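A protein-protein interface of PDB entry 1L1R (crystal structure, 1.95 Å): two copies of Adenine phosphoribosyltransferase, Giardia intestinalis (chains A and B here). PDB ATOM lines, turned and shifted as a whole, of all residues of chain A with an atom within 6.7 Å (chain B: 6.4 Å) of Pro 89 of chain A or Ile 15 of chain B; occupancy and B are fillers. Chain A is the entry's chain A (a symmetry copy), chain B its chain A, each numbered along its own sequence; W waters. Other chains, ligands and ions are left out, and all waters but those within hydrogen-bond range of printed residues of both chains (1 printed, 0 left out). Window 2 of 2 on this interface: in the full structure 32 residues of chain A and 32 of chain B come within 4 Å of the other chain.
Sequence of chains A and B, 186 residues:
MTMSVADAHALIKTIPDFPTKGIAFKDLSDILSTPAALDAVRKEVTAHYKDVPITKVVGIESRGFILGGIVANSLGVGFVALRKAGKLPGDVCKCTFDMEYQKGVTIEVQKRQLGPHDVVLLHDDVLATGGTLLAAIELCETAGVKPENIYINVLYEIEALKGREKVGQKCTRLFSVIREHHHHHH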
ATOM      1  N   GLY A  86      -2.436  17.433 -13.944  1.00  0.00           N
ATOM      2  CA  GLY A  86      -2.129  16.301 -14.799  1.00  0.00           C
ATOM      3  C   GLY A  86      -3.229  15.275 -14.950  1.00  0.00           C
ATOM      4  O   GLY A  86      -3.071  14.294 -15.675  1.00  0.00           O
ATOM      5  N   LYS A  87      -4.360  15.498 -14.294  1.00  0.00           N
ATOM      6  CA  LYS A  87      -5.444  14.536 -14.362  1.00  0.00           C
ATOM      7  C   LYS A  87      -6.582  14.913 -15.300  1.00  0.00           C
ATOM      8  O   LYS A  87      -7.143  14.052 -15.969  1.00  0.00           O
ATOM      9  CB  LYS A  87      -5.949  14.284 -12.948  1.00  0.00           C
ATOM     10  CG  LYS A  87      -4.811  13.866 -12.021  1.00  0.00           C
ATOM     11  CD  LYS A  87      -5.265  13.642 -10.596  1.00  0.00           C
ATOM     12  CE  LYS A  87      -4.074  13.291  -9.701  1.00  0.00           C
ATOM     13  NZ  LYS A  87      -4.487  12.834  -8.343  1.00  0.00           N
ATOM     14  N   LEU A  88      -6.913  16.195 -15.369  1.00  0.00           N
ATOM     15  CA  LEU A  88      -7.991  16.645 -16.241  1.00  0.00           C
ATOM     16  C   LEU A  88      -7.542  16.872 -17.679  1.00  0.00           C
ATOM     17  O   LEU A  88      -6.558  17.563 -17.925  1.00  0.00           O
ATOM     18  CB  LEU A  88      -8.581  17.952 -15.709  1.00  0.00           C
ATOM     19  CG  LEU A  88      -9.298  17.937 -14.357  1.00  0.00           C
ATOM     20  CD1 LEU A  88      -9.497  19.349 -13.878  1.00  0.00           C
ATOM     21  CD2 LEU A  88     -10.640  17.221 -14.495  1.00  0.00           C
ATOM     22  N   PRO A  89      -8.249  16.280 -18.651  1.00  0.00           N
ATOM     23  CA  PRO A  89      -7.872  16.475 -20.056  1.00  0.00           C
ATOM     24  C   PRO A  89      -8.451  17.817 -20.532  1.00  0.00           C
ATOM     25  O   PRO A  89      -9.192  18.465 -19.793  1.00  0.00           O
ATOM     26  CB  PRO A  89      -8.518  15.274 -20.751  1.00  0.00           C
ATOM     27  CG  PRO A  89      -9.774  15.074 -19.951  1.00  0.00           C
ATOM     28  CD  PRO A  89      -9.280  15.234 -18.519  1.00  0.00           C
ATOM     29  N   GLY A  90      -8.102  18.245 -21.745  1.00  0.00           N
ATOM     30  CA  GLY A  90      -8.627  19.501 -22.263  1.00  0.00           C
ATOM     31  C   GLY A  90      -8.051  20.772 -21.656  1.00  0.00           C
ATOM     32  O   GLY A  90      -7.141  20.715 -20.822  1.00  0.00           O
ATOM     33  N   ASP A  91      -8.586  21.920 -22.074  1.00  0.00           N
ATOM     34  CA  ASP A  91      -8.120  23.216 -21.583  1.00  0.00           C
ATOM     35  C   ASP A  91      -8.420  23.372 -20.107  1.00  0.00           C
ATOM     36  O   ASP A  91      -9.543  23.139 -19.654  1.00  0.00           O
ATOM     37  CB  ASP A  91      -8.767  24.363 -22.361  1.00  0.00           C
ATOM     38  CG  ASP A  91      -8.495  24.280 -23.850  1.00  0.00           C
ATOM     39  OD1 ASP A  91      -7.441  23.729 -24.243  1.00  0.00           O
ATOM     40  OD2 ASP A  91      -9.333  24.776 -24.631  1.00  0.00           O
ATOM     41  N   VAL A  92      -7.410  23.790 -19.356  1.00  0.00           N
ATOM     42  CA  VAL A  92      -7.561  23.931 -17.927  1.00  0.00           C
ATOM     43  C   VAL A  92      -6.911  25.184 -17.367  1.00  0.00           C
ATOM     44  O   VAL A  92      -5.993  25.742 -17.959  1.00  0.00           O
ATOM     45  CB  VAL A  92      -6.941  22.704 -17.216  1.00  0.00           C
ATOM     46  CG1 VAL A  92      -7.008  22.876 -15.729  1.00  0.00           C
ATOM     47  CG2 VAL A  92      -7.680  21.436 -17.612  1.00  0.00           C
ATOM     48  N   GLN A 110     -11.298  22.409 -15.497  1.00  0.00           N
ATOM     49  CA  GLN A 110     -11.543  22.561 -16.920  1.00  0.00           C
ATOM     50  C   GLN A 110     -12.191  23.909 -17.191  1.00  0.00           C
ATOM     51  O   GLN A 110     -13.191  24.265 -16.562  1.00  0.00           O
ATOM     52  CB  GLN A 110     -12.431  21.427 -17.416  1.00  0.00           C
ATOM     53  CG  GLN A 110     -11.641  20.151 -17.683  1.00  0.00           C
ATOM     54  CD  GLN A 110     -12.501  18.996 -18.140  1.00  0.00           C
ATOM     55  OE1 GLN A 110     -12.002  18.058 -18.765  1.00  0.00           O
ATOM     56  NE2 GLN A 110     -13.788  19.043 -17.821  1.00  0.00           N
ATOM     57  N   ARG A 112     -14.011  25.042 -19.611  1.00  0.00           N
ATOM     58  CA  ARG A 112     -15.394  24.953 -20.062  1.00  0.00           C
ATOM     59  C   ARG A 112     -16.451  24.697 -18.987  1.00  0.00           C
ATOM     60  O   ARG A 112     -17.630  24.978 -19.209  1.00  0.00           O
ATOM     61  CB  ARG A 112     -15.522  23.878 -21.148  1.00  0.00           C
ATOM     62  CG  ARG A 112     -15.515  22.413 -20.651  1.00  0.00           C
ATOM     63  CD  ARG A 112     -15.997  21.514 -21.794  1.00  0.00           C
ATOM     64  NE  ARG A 112     -16.113  20.104 -21.439  1.00  0.00           N
ATOM     65  CZ  ARG A 112     -15.100  19.243 -21.404  1.00  0.00           C
ATOM     66  NH1 ARG A 112     -13.869  19.635 -21.704  1.00  0.00           N
ATOM     67  NH2 ARG A 112     -15.322  17.981 -21.074  1.00  0.00           N
ATOM     68  N   LYS B  13     -16.561  13.004 -23.899  1.00  0.00           N
ATOM     69  CA  LYS B  13     -15.576  13.500 -24.856  1.00  0.00           C
ATOM     70  C   LYS B  13     -14.430  12.514 -24.954  1.00  0.00           C
ATOM     71  O   LYS B  13     -14.007  11.950 -23.953  1.00  0.00           O
ATOM     72  CB  LYS B  13     -14.994  14.860 -24.427  1.00  0.00           C
ATOM     73  CG  LYS B  13     -15.731  16.096 -24.931  1.00  0.00           C
ATOM     74  CD  LYS B  13     -17.093  16.223 -24.301  1.00  0.00           C
ATOM     75  CE  LYS B  13     -17.898  17.386 -24.866  1.00  0.00           C
ATOM     76  NZ  LYS B  13     -19.306  17.249 -24.366  1.00  0.00           N
ATOM     77  N   THR B  14     -13.924  12.315 -26.166  1.00  0.00           N
ATOM     78  CA  THR B  14     -12.805  11.414 -26.363  1.00  0.00           C
ATOM     79  C   THR B  14     -11.587  12.265 -26.677  1.00  0.00           C
ATOM     80  O   THR B  14     -11.504  12.893 -27.733  1.00  0.00           O
ATOM     81  CB  THR B  14     -13.088  10.417 -27.505  1.00  0.00           C
ATOM     82  OG1 THR B  14     -14.209   9.599 -27.146  1.00  0.00           O
ATOM     83  CG2 THR B  14     -11.880   9.512 -27.739  1.00  0.00           C
ATOM     84  N   ILE B  15     -10.660  12.306 -25.728  1.00  0.00           N
ATOM     85  CA  ILE B  15      -9.443  13.091 -25.871  1.00  0.00           C
ATOM     86  C   ILE B  15      -8.293  12.170 -26.247  1.00  0.00           C
ATOM     87  O   ILE B  15      -7.904  11.303 -25.466  1.00  0.00           O
ATOM     88  CB  ILE B  15      -9.088  13.807 -24.551  1.00  0.00           C
ATOM     89  CG1 ILE B  15     -10.312  14.555 -24.014  1.00  0.00           C
ATOM     90  CG2 ILE B  15      -7.927  14.765 -24.780  1.00  0.00           C
ATOM     91  CD1 ILE B  15     -10.826  15.645 -24.928  1.00  0.00           C
ATOM     92  N   PRO B  16      -7.729  12.347 -27.451  1.00  0.00           N
ATOM     93  CA  PRO B  16      -6.615  11.504 -27.900  1.00  0.00           C
ATOM     94  C   PRO B  16      -5.278  11.832 -27.234  1.00  0.00           C
ATOM     95  O   PRO B  16      -5.004  12.981 -26.892  1.00  0.00           O
ATOM     96  CB  PRO B  16      -6.590  11.753 -29.403  1.00  0.00           C
ATOM     97  CG  PRO B  16      -6.969  13.204 -29.491  1.00  0.00           C
ATOM     98  CD  PRO B  16      -8.117  13.313 -28.496  1.00  0.00           C
ATOM     99  N   ASP B  17      -4.455  10.809 -27.046  1.00  0.00           N
ATOM    100  CA  ASP B  17      -3.141  10.975 -26.430  1.00  0.00           C
ATOM    101  C   ASP B  17      -3.174  11.564 -25.020  1.00  0.00           C
ATOM    102  O   ASP B  17      -2.435  12.508 -24.718  1.00  0.00           O
ATOM    103  CB  ASP B  17      -2.236  11.852 -27.307  1.00  0.00           C
ATOM    104  CG  ASP B  17      -1.985  11.254 -28.683  1.00  0.00           C
ATOM    105  OD1 ASP B  17      -1.629  10.057 -28.765  1.00  0.00           O
ATOM    106  OD2 ASP B  17      -2.132  11.994 -29.681  1.00  0.00           O
ATOM    107  N   PHE B  18      -4.019  11.011 -24.154  1.00  0.00           N
ATOM    108  CA  PHE B  18      -4.099  11.490 -22.779  1.00  0.00           C
ATOM    109  C   PHE B  18      -4.337  10.346 -21.797  1.00  0.00           C
ATOM    110  O   PHE B  18      -5.146   9.460 -22.060  1.00  0.00           O
ATOM    111  CB  PHE B  18      -5.223  12.513 -22.618  1.00  0.00           C
ATOM    112  CG  PHE B  18      -5.232  13.166 -21.268  1.00  0.00           C
ATOM    113  CD1 PHE B  18      -4.376  14.229 -20.994  1.00  0.00           C
ATOM    114  CD2 PHE B  18      -6.036  12.673 -20.244  1.00  0.00           C
ATOM    115  CE1 PHE B  18      -4.315  14.792 -19.716  1.00  0.00           C
ATOM    116  CE2 PHE B  18      -5.982  13.231 -18.963  1.00  0.00           C
ATOM    117  CZ  PHE B  18      -5.118  14.292 -18.704  1.00  0.00           C
ATOM    118  N   ILE B  23      -3.016   6.481 -25.401  1.00  0.00           N
ATOM    119  CA  ILE B  23      -4.244   6.238 -24.655  1.00  0.00           C
ATOM    120  C   ILE B  23      -5.325   7.247 -25.036  1.00  0.00           C
ATOM    121  O   ILE B  23      -5.121   8.458 -24.938  1.00  0.00           O
ATOM    122  CB  ILE B  23      -4.006   6.338 -23.121  1.00  0.00           C
ATOM    123  CG1 ILE B  23      -3.126   5.175 -22.635  1.00  0.00           C
ATOM    124  CG2 ILE B  23      -5.344   6.345 -22.386  1.00  0.00           C
ATOM    125  CD1 ILE B  23      -1.664   5.261 -23.061  1.00  0.00           C
ATOM    126  N   ALA B  24      -6.469   6.743 -25.484  1.00  0.00           N
ATOM    127  CA  ALA B  24      -7.585   7.605 -25.850  1.00  0.00           C
ATOM    128  C   ALA B  24      -8.467   7.760 -24.608  1.00  0.00           C
ATOM    129  O   ALA B  24      -9.275   6.887 -24.291  1.00  0.00           O
ATOM    130  CB  ALA B  24      -8.372   6.982 -26.980  1.00  0.00           C
ATOM    131  N   PHE B  25      -8.298   8.876 -23.907  1.00  0.00           N
ATOM    132  CA  PHE B  25      -9.043   9.148 -22.684  1.00  0.00           C
ATOM    133  C   PHE B  25     -10.522   9.449 -22.918  1.00  0.00           C
ATOM    134  O   PHE B  25     -10.878  10.276 -23.751  1.00  0.00           O
ATOM    135  CB  PHE B  25      -8.399  10.322 -21.951  1.00  0.00           C
ATOM    136  CG  PHE B  25      -8.809  10.442 -20.510  1.00  0.00           C
ATOM    137  CD1 PHE B  25      -8.150   9.714 -19.526  1.00  0.00           C
ATOM    138  CD2 PHE B  25      -9.849  11.293 -20.135  1.00  0.00           C
ATOM    139  CE1 PHE B  25      -8.514   9.832 -18.175  1.00  0.00           C
ATOM    140  CE2 PHE B  25     -10.227  11.422 -18.788  1.00  0.00           C
ATOM    141  CZ  PHE B  25      -9.557  10.690 -17.807  1.00  0.00           C
ATOM    142  N   LYS B  26     -11.377   8.755 -22.179  1.00  0.00           N
ATOM    143  CA  LYS B  26     -12.812   8.960 -22.256  1.00  0.00           C
ATOM    144  C   LYS B  26     -13.150   9.905 -21.099  1.00  0.00           C
ATOM    145  O   LYS B  26     -13.130   9.507 -19.936  1.00  0.00           O
ATOM    146  CB  LYS B  26     -13.538   7.626 -22.087  1.00  0.00           C
ATOM    147  CG  LYS B  26     -13.403   6.680 -23.270  1.00  0.00           C
ATOM    148  CD  LYS B  26     -14.194   7.185 -24.472  1.00  0.00           C
ATOM    149  CE  LYS B  26     -14.046   6.268 -25.680  1.00  0.00           C
ATOM    150  NZ  LYS B  26     -14.939   6.687 -26.803  1.00  0.00           N
ATOM    151  N   ASP B  27     -13.435  11.159 -21.435  1.00  0.00           N
ATOM    152  CA  ASP B  27     -13.752  12.193 -20.451  1.00  0.00           C
ATOM    153  C   ASP B  27     -15.258  12.228 -20.159  1.00  0.00           C
ATOM    154  O   ASP B  27     -16.043  12.642 -20.994  1.00  0.00           O
ATOM    155  CB  ASP B  27     -13.257  13.548 -20.994  1.00  0.00           C
ATOM    156  CG  ASP B  27     -13.517  14.695 -20.043  1.00  0.00           C
ATOM    157  OD1 ASP B  27     -13.704  14.427 -18.840  1.00  0.00           O
ATOM    158  OD2 ASP B  27     -13.514  15.859 -20.503  1.00  0.00           O
HETATM  159  O   HOH W   1     -11.962  17.591 -22.196  1.00  0.00           O
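No position is printed for both chains.
O of Gly 86 of chain A touches CZ of Phe 18 of chain B, at 3.7 Å.
O of Lys 87 of chain A touches CE2 of Phe 18 of chain B, at 3.3 Å.
Leu 88 of chain A touches Phe 18 of chain B.
Pro 89 of chain A touches Ile 15 of chain B (CB to CG1, 3.8 Å).
Pro 89 of chain A touches Phe 18 of chain B.
Phe 25 of chain B touches Pro 89 of chain A.
Asp 27 of chain B touches Pro 89 of chain A (CG to CG, 3.8 Å).
The backbone NH of Asp 27 of chain B sits at hydrogen-bond distance from the backbone carbonyl oxygen of Lys 13 of chain B (2.7 Å).
The backbone carbonyl oxygen (O) of Phe 25 of chain B sits at hydrogen-bond distance from the backbone NH (N) of Ile 15 of chain B, at 2.8 Å.
The backbone carbonyl oxygen (O) of Ile 23 of chain B lies within hydrogen-bond range of the backbone NH (N) of Phe 18 of chain B (2.9 Å).
O of Pro 89 of chain A sits close to OE1 of Gln 110 of chain A (3.0 Å).
Water W1 lies within hydrogen-bond range of NH1 of Arg 112 of chain A (2.8 Å), OD2 of Asp 27 of chain B (2.9 Å) and OE1 of Gln 110 of chain A (3.5 Å).
The side-chain amide oxygen of Gln 110 of chain A lies close to the side-chain carboxylate of Asp 27 of chain B.
OD2 of Asp 27 of chain B is in salt-bridge range of NH2 of Arg 112 of chain A (2.8 Å).
Printed residues of chain B within 4 Å of Leu 88 of chain A: Phe 18 (3.7 Å).
Pro 89 of chain A touches just these residues of chain B: Ile 15, Phe 18, Phe 25 and Asp 27.
Printed residues of chain B within 4 Å of Gln 110 of chain A: Asp 27 (3.2 Å).
Printed residues of chain B within 4 Å of Arg 112 of chain A: Asp 27 (2.8 Å).
Of chain A, only Pro 89 (3.8 Å) comes within 4 Å of Ile 15 of chain B.
Asp 17 of chain B touches none of the printed residues of chain A.
Of the printed residues of chain A, Phe 18 of chain B touches Gly 86 (3.7 Å), Lys 87 (3.3 Å), Leu 88 (3.7 Å) and Pro 89 (3.6 Å).
Ile 23 of chain B touches none of the printed residues of chain A.
Printed residues of chain A within 4 Å of Phe 25 of chain B: Pro 89.
The nearest residue of chain B that does not touch Pro 89 of chain A is Lys 26 of chain B (6.3 Å).
The nearest residue of chain A that does not touch Ile 15 of chain B is Gly 90 of chain A (4.6 Å).
Of the 11 printed residues of chain B, 4 touch a printed residue of chain A.
Hydrophobic or aromatic side chains of chain B that line the printed part of chain A: Ile 15, Phe 18 and Phe 25.
Among the printed residues, 9 pairs touch across the chains.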
